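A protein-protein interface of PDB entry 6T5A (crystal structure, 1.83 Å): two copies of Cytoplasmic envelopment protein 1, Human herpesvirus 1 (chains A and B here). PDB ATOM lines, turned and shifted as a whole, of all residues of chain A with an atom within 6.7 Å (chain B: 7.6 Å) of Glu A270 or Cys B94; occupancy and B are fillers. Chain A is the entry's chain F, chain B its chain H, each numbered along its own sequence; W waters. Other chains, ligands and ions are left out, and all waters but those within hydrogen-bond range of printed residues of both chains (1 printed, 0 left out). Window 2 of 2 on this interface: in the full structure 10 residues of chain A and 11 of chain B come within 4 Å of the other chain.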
ATOM      1  N   SER A 116      -0.999  35.539  14.144  1.00  0.00           N
ATOM      2  CA  SER A 116      -1.230  34.961  12.822  1.00  0.00           C
ATOM      3  C   SER A 116      -2.718  34.969  12.524  1.00  0.00           C
ATOM      4  O   SER A 116      -3.541  35.211  13.422  1.00  0.00           O
ATOM      5  CB  SER A 116      -0.706  33.525  12.778  1.00  0.00           C
ATOM      6  OG  SER A 116      -1.415  32.685  13.677  1.00  0.00           O
ATOM      7  N   LEU A 117      -3.064  34.691  11.260  1.00  0.00           N
ATOM      8  CA  LEU A 117      -4.451  34.532  10.826  1.00  0.00           C
ATOM      9  C   LEU A 117      -4.585  33.077  10.410  1.00  0.00           C
ATOM     10  O   LEU A 117      -3.669  32.546   9.768  1.00  0.00           O
ATOM     11  CB  LEU A 117      -4.808  35.465   9.657  1.00  0.00           C
ATOM     12  CG  LEU A 117      -4.649  36.993   9.869  1.00  0.00           C
ATOM     13  CD1 LEU A 117      -5.153  37.756   8.628  1.00  0.00           C
ATOM     14  CD2 LEU A 117      -5.420  37.488  11.115  1.00  0.00           C
ATOM     15  N   VAL A 119      -5.866  31.639   8.106  1.00  0.00           N
ATOM     16  CA  VAL A 119      -6.282  31.705   6.715  1.00  0.00           C
ATOM     17  C   VAL A 119      -5.025  31.457   5.880  1.00  0.00           C
ATOM     18  O   VAL A 119      -4.117  32.289   5.940  1.00  0.00           O
ATOM     19  CB  VAL A 119      -6.946  33.077   6.364  1.00  0.00           C
ATOM     20  CG1 VAL A 119      -7.401  33.112   4.905  1.00  0.00           C
ATOM     21  CG2 VAL A 119      -8.126  33.393   7.292  1.00  0.00           C
ATOM     22  N   PRO A 120      -4.922  30.336   5.109  1.00  0.00           N
ATOM     23  CA  PRO A 120      -3.715  30.130   4.286  1.00  0.00           C
ATOM     24  C   PRO A 120      -3.425  31.319   3.357  1.00  0.00           C
ATOM     25  O   PRO A 120      -4.364  31.967   2.902  1.00  0.00           O
ATOM     26  CB  PRO A 120      -4.032  28.837   3.509  1.00  0.00           C
ATOM     27  CG  PRO A 120      -5.024  28.126   4.367  1.00  0.00           C
ATOM     28  CD  PRO A 120      -5.876  29.219   4.936  1.00  0.00           C
ATOM     29  N   PRO A 121      -2.136  31.636   3.057  1.00  0.00           N
ATOM     30  CA  PRO A 121      -1.839  32.824   2.211  1.00  0.00           C
ATOM     31  C   PRO A 121      -2.577  32.906   0.869  1.00  0.00           C
ATOM     32  O   PRO A 121      -2.970  33.996   0.458  1.00  0.00           O
ATOM     33  CB  PRO A 121      -0.308  32.770   2.000  1.00  0.00           C
ATOM     34  CG  PRO A 121       0.153  31.522   2.633  1.00  0.00           C
ATOM     35  CD  PRO A 121      -0.902  30.997   3.556  1.00  0.00           C
ATOM     36  N   LEU A 122      -2.770  31.767   0.186  1.00  0.00           N
ATOM     37  CA  LEU A 122      -3.465  31.749  -1.100  1.00  0.00           C
ATOM     38  C   LEU A 122      -4.969  31.952  -0.950  1.00  0.00           C
ATOM     39  O   LEU A 122      -5.613  32.404  -1.886  1.00  0.00           O
ATOM     40  CB  LEU A 122      -3.123  30.499  -1.930  1.00  0.00           C
ATOM     41  CG  LEU A 122      -1.650  30.423  -2.382  1.00  0.00           C
ATOM     42  CD1 LEU A 122      -1.351  29.117  -3.068  1.00  0.00           C
ATOM     43  CD2 LEU A 122      -1.277  31.595  -3.302  1.00  0.00           C
ATOM     44  N   LEU A 124      -6.107  33.948   1.733  1.00  0.00           N
ATOM     45  CA  LEU A 124      -6.120  35.353   2.156  1.00  0.00           C
ATOM     46  C   LEU A 124      -6.132  36.315   0.969  1.00  0.00           C
ATOM     47  O   LEU A 124      -6.789  37.355   1.012  1.00  0.00           O
ATOM     48  CB  LEU A 124      -4.969  35.664   3.139  1.00  0.00           C
ATOM     49  CG  LEU A 124      -5.068  37.016   3.876  1.00  0.00           C
ATOM     50  CD1 LEU A 124      -6.324  37.081   4.781  1.00  0.00           C
ATOM     51  CD2 LEU A 124      -3.799  37.282   4.690  1.00  0.00           C
ATOM     52  N   CYS A 234       1.213  31.472  17.080  1.00  0.00           N
ATOM     53  CA  CYS A 234       2.450  31.772  16.339  1.00  0.00           C
ATOM     54  C   CYS A 234       3.103  33.036  16.888  1.00  0.00           C
ATOM     55  O   CYS A 234       4.298  33.259  16.714  1.00  0.00           O
ATOM     56  CB  CYS A 234       2.222  31.857  14.834  1.00  0.00           C
ATOM     57  SG  CYS A 234       1.587  30.330  14.100  1.00  0.00           S
ATOM     58  N   CYS A 265      -0.918  40.839  13.807  1.00  0.00           N
ATOM     59  CA  CYS A 265      -1.102  40.003  12.594  1.00  0.00           C
ATOM     60  C   CYS A 265      -0.255  40.484  11.423  1.00  0.00           C
ATOM     61  O   CYS A 265       0.084  39.676  10.554  1.00  0.00           O
ATOM     62  CB  CYS A 265      -2.569  39.888  12.189  1.00  0.00           C
ATOM     63  SG  CYS A 265      -3.513  41.426  12.370  1.00  0.00           S
ATOM     64  N   ALA A 267       2.867  41.365  11.397  1.00  0.00           N
ATOM     65  CA  ALA A 267       4.252  40.862  11.453  1.00  0.00           C
ATOM     66  C   ALA A 267       4.494  39.651  10.534  1.00  0.00           C
ATOM     67  O   ALA A 267       5.594  39.494  10.007  1.00  0.00           O
ATOM     68  CB  ALA A 267       4.623  40.517  12.889  1.00  0.00           C
ATOM     69  N   SER A 268       3.454  38.822  10.335  1.00  0.00           N
ATOM     70  CA  SER A 268       3.474  37.602   9.532  1.00  0.00           C
ATOM     71  C   SER A 268       3.667  37.866   8.032  1.00  0.00           C
ATOM     72  O   SER A 268       2.929  38.656   7.428  1.00  0.00           O
ATOM     73  CB  SER A 268       2.190  36.812   9.779  1.00  0.00           C
ATOM     74  OG  SER A 268       2.113  35.638   8.991  1.00  0.00           O
ATOM     75  N   GLU A 269       4.652  37.176   7.429  1.00  0.00           N
ATOM     76  CA  GLU A 269       4.931  37.225   5.990  1.00  0.00           C
ATOM     77  C   GLU A 269       3.747  36.564   5.236  1.00  0.00           C
ATOM     78  O   GLU A 269       3.486  36.907   4.089  1.00  0.00           O
ATOM     79  CB  GLU A 269       6.254  36.507   5.678  1.00  0.00           C
ATOM     80  CG  GLU A 269       6.703  36.554   4.219  1.00  0.00           C
ATOM     81  CD  GLU A 269       7.288  37.840   3.654  1.00  0.00           C
ATOM     82  OE1 GLU A 269       7.200  38.900   4.314  1.00  0.00           O
ATOM     83  OE2 GLU A 269       7.835  37.781   2.528  1.00  0.00           O
ATOM     84  N   GLU A 270       3.015  35.649   5.910  1.00  0.00           N
ATOM     85  CA  GLU A 270       1.837  34.966   5.367  1.00  0.00           C
ATOM     86  C   GLU A 270       0.608  35.890   5.320  1.00  0.00           C
ATOM     87  O   GLU A 270      -0.454  35.476   4.860  1.00  0.00           O
ATOM     88  CB  GLU A 270       1.547  33.672   6.145  1.00  0.00           C
ATOM     89  CG  GLU A 270       2.538  32.567   5.809  1.00  0.00           C
ATOM     90  CD  GLU A 270       2.188  31.182   6.316  1.00  0.00           C
ATOM     91  OE1 GLU A 270       1.772  31.062   7.492  1.00  0.00           O
ATOM     92  OE2 GLU A 270       2.350  30.211   5.540  1.00  0.00           O
ATOM     93  N   VAL A 271       0.768  37.142   5.800  1.00  0.00           N
ATOM     94  CA  VAL A 271      -0.243  38.197   5.781  1.00  0.00           C
ATOM     95  C   VAL A 271       0.184  39.284   4.764  1.00  0.00           C
ATOM     96  O   VAL A 271      -0.612  39.644   3.895  1.00  0.00           O
ATOM     97  CB  VAL A 271      -0.515  38.776   7.204  1.00  0.00           C
ATOM     98  CG1 VAL A 271      -1.186  40.143   7.133  1.00  0.00           C
ATOM     99  CG2 VAL A 271      -1.354  37.816   8.051  1.00  0.00           C
ATOM    100  N   ARG A 272       1.451  39.762   4.844  1.00  0.00           N
ATOM    101  CA  ARG A 272       1.978  40.834   3.977  1.00  0.00           C
ATOM    102  C   ARG A 272       2.240  40.430   2.527  1.00  0.00           C
ATOM    103  O   ARG A 272       1.945  41.229   1.636  1.00  0.00           O
ATOM    104  CB  ARG A 272       3.228  41.485   4.582  1.00  0.00           C
ATOM    105  CG  ARG A 272       2.907  42.292   5.846  1.00  0.00           C
ATOM    106  CD  ARG A 272       4.154  42.884   6.478  1.00  0.00           C
ATOM    107  NE  ARG A 272       4.898  41.867   7.230  1.00  0.00           N
ATOM    108  CZ  ARG A 272       6.030  41.310   6.821  1.00  0.00           C
ATOM    109  NH1 ARG A 272       6.591  41.689   5.681  1.00  0.00           N
ATOM    110  NH2 ARG A 272       6.622  40.379   7.555  1.00  0.00           N
ATOM    111  N   ALA A 273       2.823  39.236   2.272  1.00  0.00           N
ATOM    112  CA  ALA A 273       3.064  38.806   0.881  1.00  0.00           C
ATOM    113  C   ALA A 273       1.732  38.662   0.107  1.00  0.00           C
ATOM    114  O   ALA A 273       1.644  39.242  -0.970  1.00  0.00           O
ATOM    115  CB  ALA A 273       3.902  37.530   0.821  1.00  0.00           C
ATOM    116  N   PRO A 274       0.641  38.059   0.666  1.00  0.00           N
ATOM    117  CA  PRO A 274      -0.634  38.029  -0.077  1.00  0.00           C
ATOM    118  C   PRO A 274      -1.204  39.423  -0.372  1.00  0.00           C
ATOM    119  O   PRO A 274      -1.811  39.598  -1.424  1.00  0.00           O
ATOM    120  CB  PRO A 274      -1.569  37.256   0.863  1.00  0.00           C
ATOM    121  CG  PRO A 274      -0.689  36.447   1.677  1.00  0.00           C
ATOM    122  CD  PRO A 274       0.524  37.276   1.913  1.00  0.00           C
ATOM    123  N   LEU A 275      -1.043  40.406   0.550  1.00  0.00           N
ATOM    124  CA  LEU A 275      -1.543  41.773   0.319  1.00  0.00           C
ATOM    125  C   LEU A 275      -0.891  42.386  -0.929  1.00  0.00           C
ATOM    126  O   LEU A 275      -1.593  42.897  -1.806  1.00  0.00           O
ATOM    127  CB  LEU A 275      -1.312  42.678   1.546  1.00  0.00           C
ATOM    128  CG  LEU A 275      -1.631  44.181   1.367  1.00  0.00           C
ATOM    129  CD1 LEU A 275      -3.136  44.427   1.093  1.00  0.00           C
ATOM    130  CD2 LEU A 275      -1.156  44.987   2.578  1.00  0.00           C
ATOM    131  N   GLU B  87      -0.076  17.717   8.193  1.00  0.00           N
ATOM    132  CA  GLU B  87       0.054  19.087   8.699  1.00  0.00           C
ATOM    133  C   GLU B  87       1.400  19.693   8.289  1.00  0.00           C
ATOM    134  O   GLU B  87       1.429  20.830   7.808  1.00  0.00           O
ATOM    135  CB  GLU B  87      -0.147  19.144  10.220  1.00  0.00           C
ATOM    136  CG  GLU B  87      -0.298  20.557  10.760  1.00  0.00           C
ATOM    137  CD  GLU B  87      -0.640  20.676  12.233  1.00  0.00           C
ATOM    138  OE1 GLU B  87      -1.364  19.798  12.758  1.00  0.00           O
ATOM    139  OE2 GLU B  87      -0.200  21.667  12.858  1.00  0.00           O
ATOM    140  N   ASP B  88       2.504  18.929   8.457  1.00  0.00           N
ATOM    141  CA  ASP B  88       3.843  19.401   8.095  1.00  0.00           C
ATOM    142  C   ASP B  88       3.983  19.616   6.579  1.00  0.00           C
ATOM    143  O   ASP B  88       4.627  20.583   6.173  1.00  0.00           O
ATOM    144  CB  ASP B  88       4.942  18.488   8.683  1.00  0.00           C
ATOM    145  CG  ASP B  88       5.177  18.689  10.184  1.00  0.00           C
ATOM    146  OD1 ASP B  88       4.696  19.710  10.739  1.00  0.00           O
ATOM    147  OD2 ASP B  88       5.852  17.834  10.801  1.00  0.00           O
ATOM    148  N   TYR B  89       3.328  18.767   5.757  1.00  0.00           N
ATOM    149  CA  TYR B  89       3.331  18.907   4.295  1.00  0.00           C
ATOM    150  C   TYR B  89       2.443  20.098   3.856  1.00  0.00           C
ATOM    151  O   TYR B  89       2.803  20.815   2.917  1.00  0.00           O
ATOM    152  CB  TYR B  89       2.960  17.589   3.586  1.00  0.00           C
ATOM    153  CG  TYR B  89       3.148  17.646   2.083  1.00  0.00           C
ATOM    154  CD1 TYR B  89       4.338  18.110   1.526  1.00  0.00           C
ATOM    155  CD2 TYR B  89       2.145  17.220   1.218  1.00  0.00           C
ATOM    156  CE1 TYR B  89       4.504  18.200   0.145  1.00  0.00           C
ATOM    157  CE2 TYR B  89       2.306  17.288  -0.169  1.00  0.00           C
ATOM    158  CZ  TYR B  89       3.491  17.774  -0.698  1.00  0.00           C
ATOM    159  OH  TYR B  89       3.673  17.841  -2.054  1.00  0.00           O
ATOM    160  N   PHE B  90       1.332  20.347   4.587  1.00  0.00           N
ATOM    161  CA  PHE B  90       0.442  21.498   4.362  1.00  0.00           C
ATOM    162  C   PHE B  90       1.207  22.811   4.617  1.00  0.00           C
ATOM    163  O   PHE B  90       1.167  23.707   3.769  1.00  0.00           O
ATOM    164  CB  PHE B  90      -0.824  21.401   5.250  1.00  0.00           C
ATOM    165  CG  PHE B  90      -1.904  22.450   5.067  1.00  0.00           C
ATOM    166  CD1 PHE B  90      -2.219  22.941   3.805  1.00  0.00           C
ATOM    167  CD2 PHE B  90      -2.653  22.898   6.150  1.00  0.00           C
ATOM    168  CE1 PHE B  90      -3.261  23.860   3.626  1.00  0.00           C
ATOM    169  CE2 PHE B  90      -3.681  23.838   5.973  1.00  0.00           C
ATOM    170  CZ  PHE B  90      -3.982  24.301   4.710  1.00  0.00           C
ATOM    171  N   LYS B  91       1.962  22.889   5.739  1.00  0.00           N
ATOM    172  CA  LYS B  91       2.770  24.070   6.105  1.00  0.00           C
ATOM    173  C   LYS B  91       3.891  24.324   5.086  1.00  0.00           C
ATOM    174  O   LYS B  91       4.127  25.472   4.712  1.00  0.00           O
ATOM    175  CB  LYS B  91       3.378  23.926   7.515  1.00  0.00           C
ATOM    176  CG  LYS B  91       2.366  24.021   8.651  1.00  0.00           C
ATOM    177  CD  LYS B  91       3.053  23.888  10.007  1.00  0.00           C
ATOM    178  CE  LYS B  91       2.070  23.853  11.150  1.00  0.00           C
ATOM    179  NZ  LYS B  91       2.753  23.702  12.460  1.00  0.00           N
ATOM    180  N   ARG B  92       4.577  23.250   4.645  1.00  0.00           N
ATOM    181  CA  ARG B  92       5.659  23.305   3.658  1.00  0.00           C
ATOM    182  C   ARG B  92       5.135  23.890   2.322  1.00  0.00           C
ATOM    183  O   ARG B  92       5.781  24.768   1.751  1.00  0.00           O
ATOM    184  CB  ARG B  92       6.249  21.897   3.445  1.00  0.00           C
ATOM    185  CG  ARG B  92       7.471  21.856   2.527  1.00  0.00           C
ATOM    186  CD  ARG B  92       7.835  20.448   2.097  1.00  0.00           C
ATOM    187  NE  ARG B  92       8.333  19.640   3.210  1.00  0.00           N
ATOM    188  CZ  ARG B  92       8.998  18.500   3.069  1.00  0.00           C
ATOM    189  NH1 ARG B  92       9.259  18.022   1.858  1.00  0.00           N
ATOM    190  NH2 ARG B  92       9.411  17.830   4.135  1.00  0.00           N
ATOM    191  N   CYS B  93       3.969  23.412   1.848  1.00  0.00           N
ATOM    192  CA  CYS B  93       3.348  23.896   0.607  1.00  0.00           C
ATOM    193  C   CYS B  93       2.907  25.353   0.732  1.00  0.00           C
ATOM    194  O   CYS B  93       3.179  26.143  -0.173  1.00  0.00           O
ATOM    195  CB  CYS B  93       2.202  22.990   0.170  1.00  0.00           C
ATOM    196  SG  CYS B  93       2.741  21.358  -0.406  1.00  0.00           S
ATOM    197  N   CYS B  94       2.281  25.723   1.875  1.00  0.00           N
ATOM    198  CA  CYS B  94       1.834  27.100   2.141  1.00  0.00           C
ATOM    199  C   CYS B  94       2.993  28.085   2.195  1.00  0.00           C
ATOM    200  O   CYS B  94       2.812  29.253   1.855  1.00  0.00           O
ATOM    201  CB  CYS B  94       0.976  27.177   3.402  1.00  0.00           C
ATOM    202  SG  CYS B  94      -0.652  26.403   3.231  1.00  0.00           S
ATOM    203  N   GLY B  95       4.164  27.596   2.611  1.00  0.00           N
ATOM    204  CA  GLY B  95       5.395  28.369   2.723  1.00  0.00           C
ATOM    205  C   GLY B  95       6.214  28.458   1.451  1.00  0.00           C
ATOM    206  O   GLY B  95       7.183  29.211   1.419  1.00  0.00           O
ATOM    207  N   GLN B  96       5.847  27.694   0.394  1.00  0.00           N
ATOM    208  CA  GLN B  96       6.542  27.711  -0.905  1.00  0.00           C
ATOM    209  C   GLN B  96       5.936  28.800  -1.785  1.00  0.00           C
ATOM    210  O   GLN B  96       4.760  28.704  -2.136  1.00  0.00           O
ATOM    211  CB  GLN B  96       6.395  26.370  -1.624  1.00  0.00           C
ATOM    212  CG  GLN B  96       7.314  25.249  -1.160  1.00  0.00           C
ATOM    213  CD  GLN B  96       6.807  23.901  -1.645  1.00  0.00           C
ATOM    214  OE1 GLN B  96       6.192  23.767  -2.719  1.00  0.00           O
ATOM    215  NE2 GLN B  96       7.042  22.866  -0.855  1.00  0.00           N
ATOM    216  N   SER B  97       6.728  29.828  -2.156  1.00  0.00           N
ATOM    217  CA  SER B  97       6.235  30.937  -2.991  1.00  0.00           C
ATOM    218  C   SER B  97       5.809  30.489  -4.402  1.00  0.00           C
ATOM    219  O   SER B  97       4.914  31.096  -4.983  1.00  0.00           O
ATOM    220  CB  SER B  97       7.228  32.098  -3.036  1.00  0.00           C
ATOM    221  OG  SER B  97       8.527  31.681  -3.415  1.00  0.00           O
ATOM    222  N   TYR B  99       4.337  27.521  -5.052  1.00  0.00           N
ATOM    223  CA  TYR B  99       3.124  26.717  -4.888  1.00  0.00           C
ATOM    224  C   TYR B  99       1.859  27.536  -5.161  1.00  0.00           C
ATOM    225  O   TYR B  99       1.675  28.602  -4.570  1.00  0.00           O
ATOM    226  CB  TYR B  99       3.100  26.079  -3.493  1.00  0.00           C
ATOM    227  CG  TYR B  99       1.984  25.085  -3.295  1.00  0.00           C
ATOM    228  CD1 TYR B  99       2.091  23.781  -3.776  1.00  0.00           C
ATOM    229  CD2 TYR B  99       0.826  25.437  -2.612  1.00  0.00           C
ATOM    230  CE1 TYR B  99       1.064  22.859  -3.597  1.00  0.00           C
ATOM    231  CE2 TYR B  99      -0.203  24.523  -2.418  1.00  0.00           C
ATOM    232  CZ  TYR B  99      -0.083  23.239  -2.922  1.00  0.00           C
ATOM    233  OH  TYR B  99      -1.089  22.335  -2.717  1.00  0.00           O
ATOM    234  N   PRO B 133      -6.565  24.908  -0.620  1.00  0.00           N
ATOM    235  CA  PRO B 133      -7.116  24.347   0.624  1.00  0.00           C
ATOM    236  C   PRO B 133      -7.282  25.389   1.729  1.00  0.00           C
ATOM    237  O   PRO B 133      -6.383  26.180   1.993  1.00  0.00           O
ATOM    238  CB  PRO B 133      -6.124  23.237   0.975  1.00  0.00           C
ATOM    239  CG  PRO B 133      -5.578  22.821  -0.341  1.00  0.00           C
ATOM    240  CD  PRO B 133      -5.418  24.106  -1.094  1.00  0.00           C
ATOM    241  N   PHE B 139      -6.808  20.007   2.435  1.00  0.00           N
ATOM    242  CA  PHE B 139      -5.499  19.630   1.889  1.00  0.00           C
ATOM    243  C   PHE B 139      -5.346  18.102   1.821  1.00  0.00           C
ATOM    244  O   PHE B 139      -4.893  17.588   0.799  1.00  0.00           O
ATOM    245  CB  PHE B 139      -4.376  20.248   2.725  1.00  0.00           C
ATOM    246  CG  PHE B 139      -2.982  20.011   2.200  1.00  0.00           C
ATOM    247  CD1 PHE B 139      -2.485  20.762   1.142  1.00  0.00           C
ATOM    248  CD2 PHE B 139      -2.150  19.064   2.791  1.00  0.00           C
ATOM    249  CE1 PHE B 139      -1.189  20.566   0.678  1.00  0.00           C
ATOM    250  CE2 PHE B 139      -0.857  18.855   2.315  1.00  0.00           C
ATOM    251  CZ  PHE B 139      -0.387  19.603   1.255  1.00  0.00           C
HETATM  252  O   HOH W   1       3.602  27.738   6.133  1.00  0.00           O
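The side-chain hydroxyl of Ser A268 sits close to the backbone NH of Glu A270.
The side-chain sulfur of Cys B94 sits at hydrogen-bond distance from the backbone carbonyl oxygen of Phe B90.
Among the printed residues, merely in contact across the chains: Pro A120 with Phe B90 (3.98 Å), Pro A120 with Pro B133 (3.4 Å), Pro A121 with Cys B94 (3.6 Å), Leu A122 with Tyr B99 (3.4 Å) and Glu A270 with Cys B94 (3.8 Å).
Cys B94 touches two residues of chain A.
Of the printed residues of chain B, Pro A120 touches Phe B90 and Pro B133.
Printed residues of chain B within 4 Å of Leu A122: Tyr B99.
Of the printed residues of chain B, Pro A121 touches Cys B94 (3.6 Å).
Of the printed residues of chain A, Phe B90 touches Pro A120.
Of the printed residues of chain A, Pro B133 touches Pro A120.
Phe B139 touches none of the printed residues of chain A.
The nearest residue of chain B that does not touch Glu A270 is Gly B95 (4.3 Å).
The nearest printed residue of chain A that does not touch Pro B133 is Leu A122 (6.6 Å).
Printed residues of chain A that touch a printed residue of chain B: Pro A120, Pro A121, Leu A122 and Glu A270.
Among the printed residues, 5 pairs touch across the chains.
No position is printed for both chains.
Water W1 lies within hydrogen-bond range of O of Lys B91 (2.7 Å) and OE2 of Glu A270 (2.8 Å).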
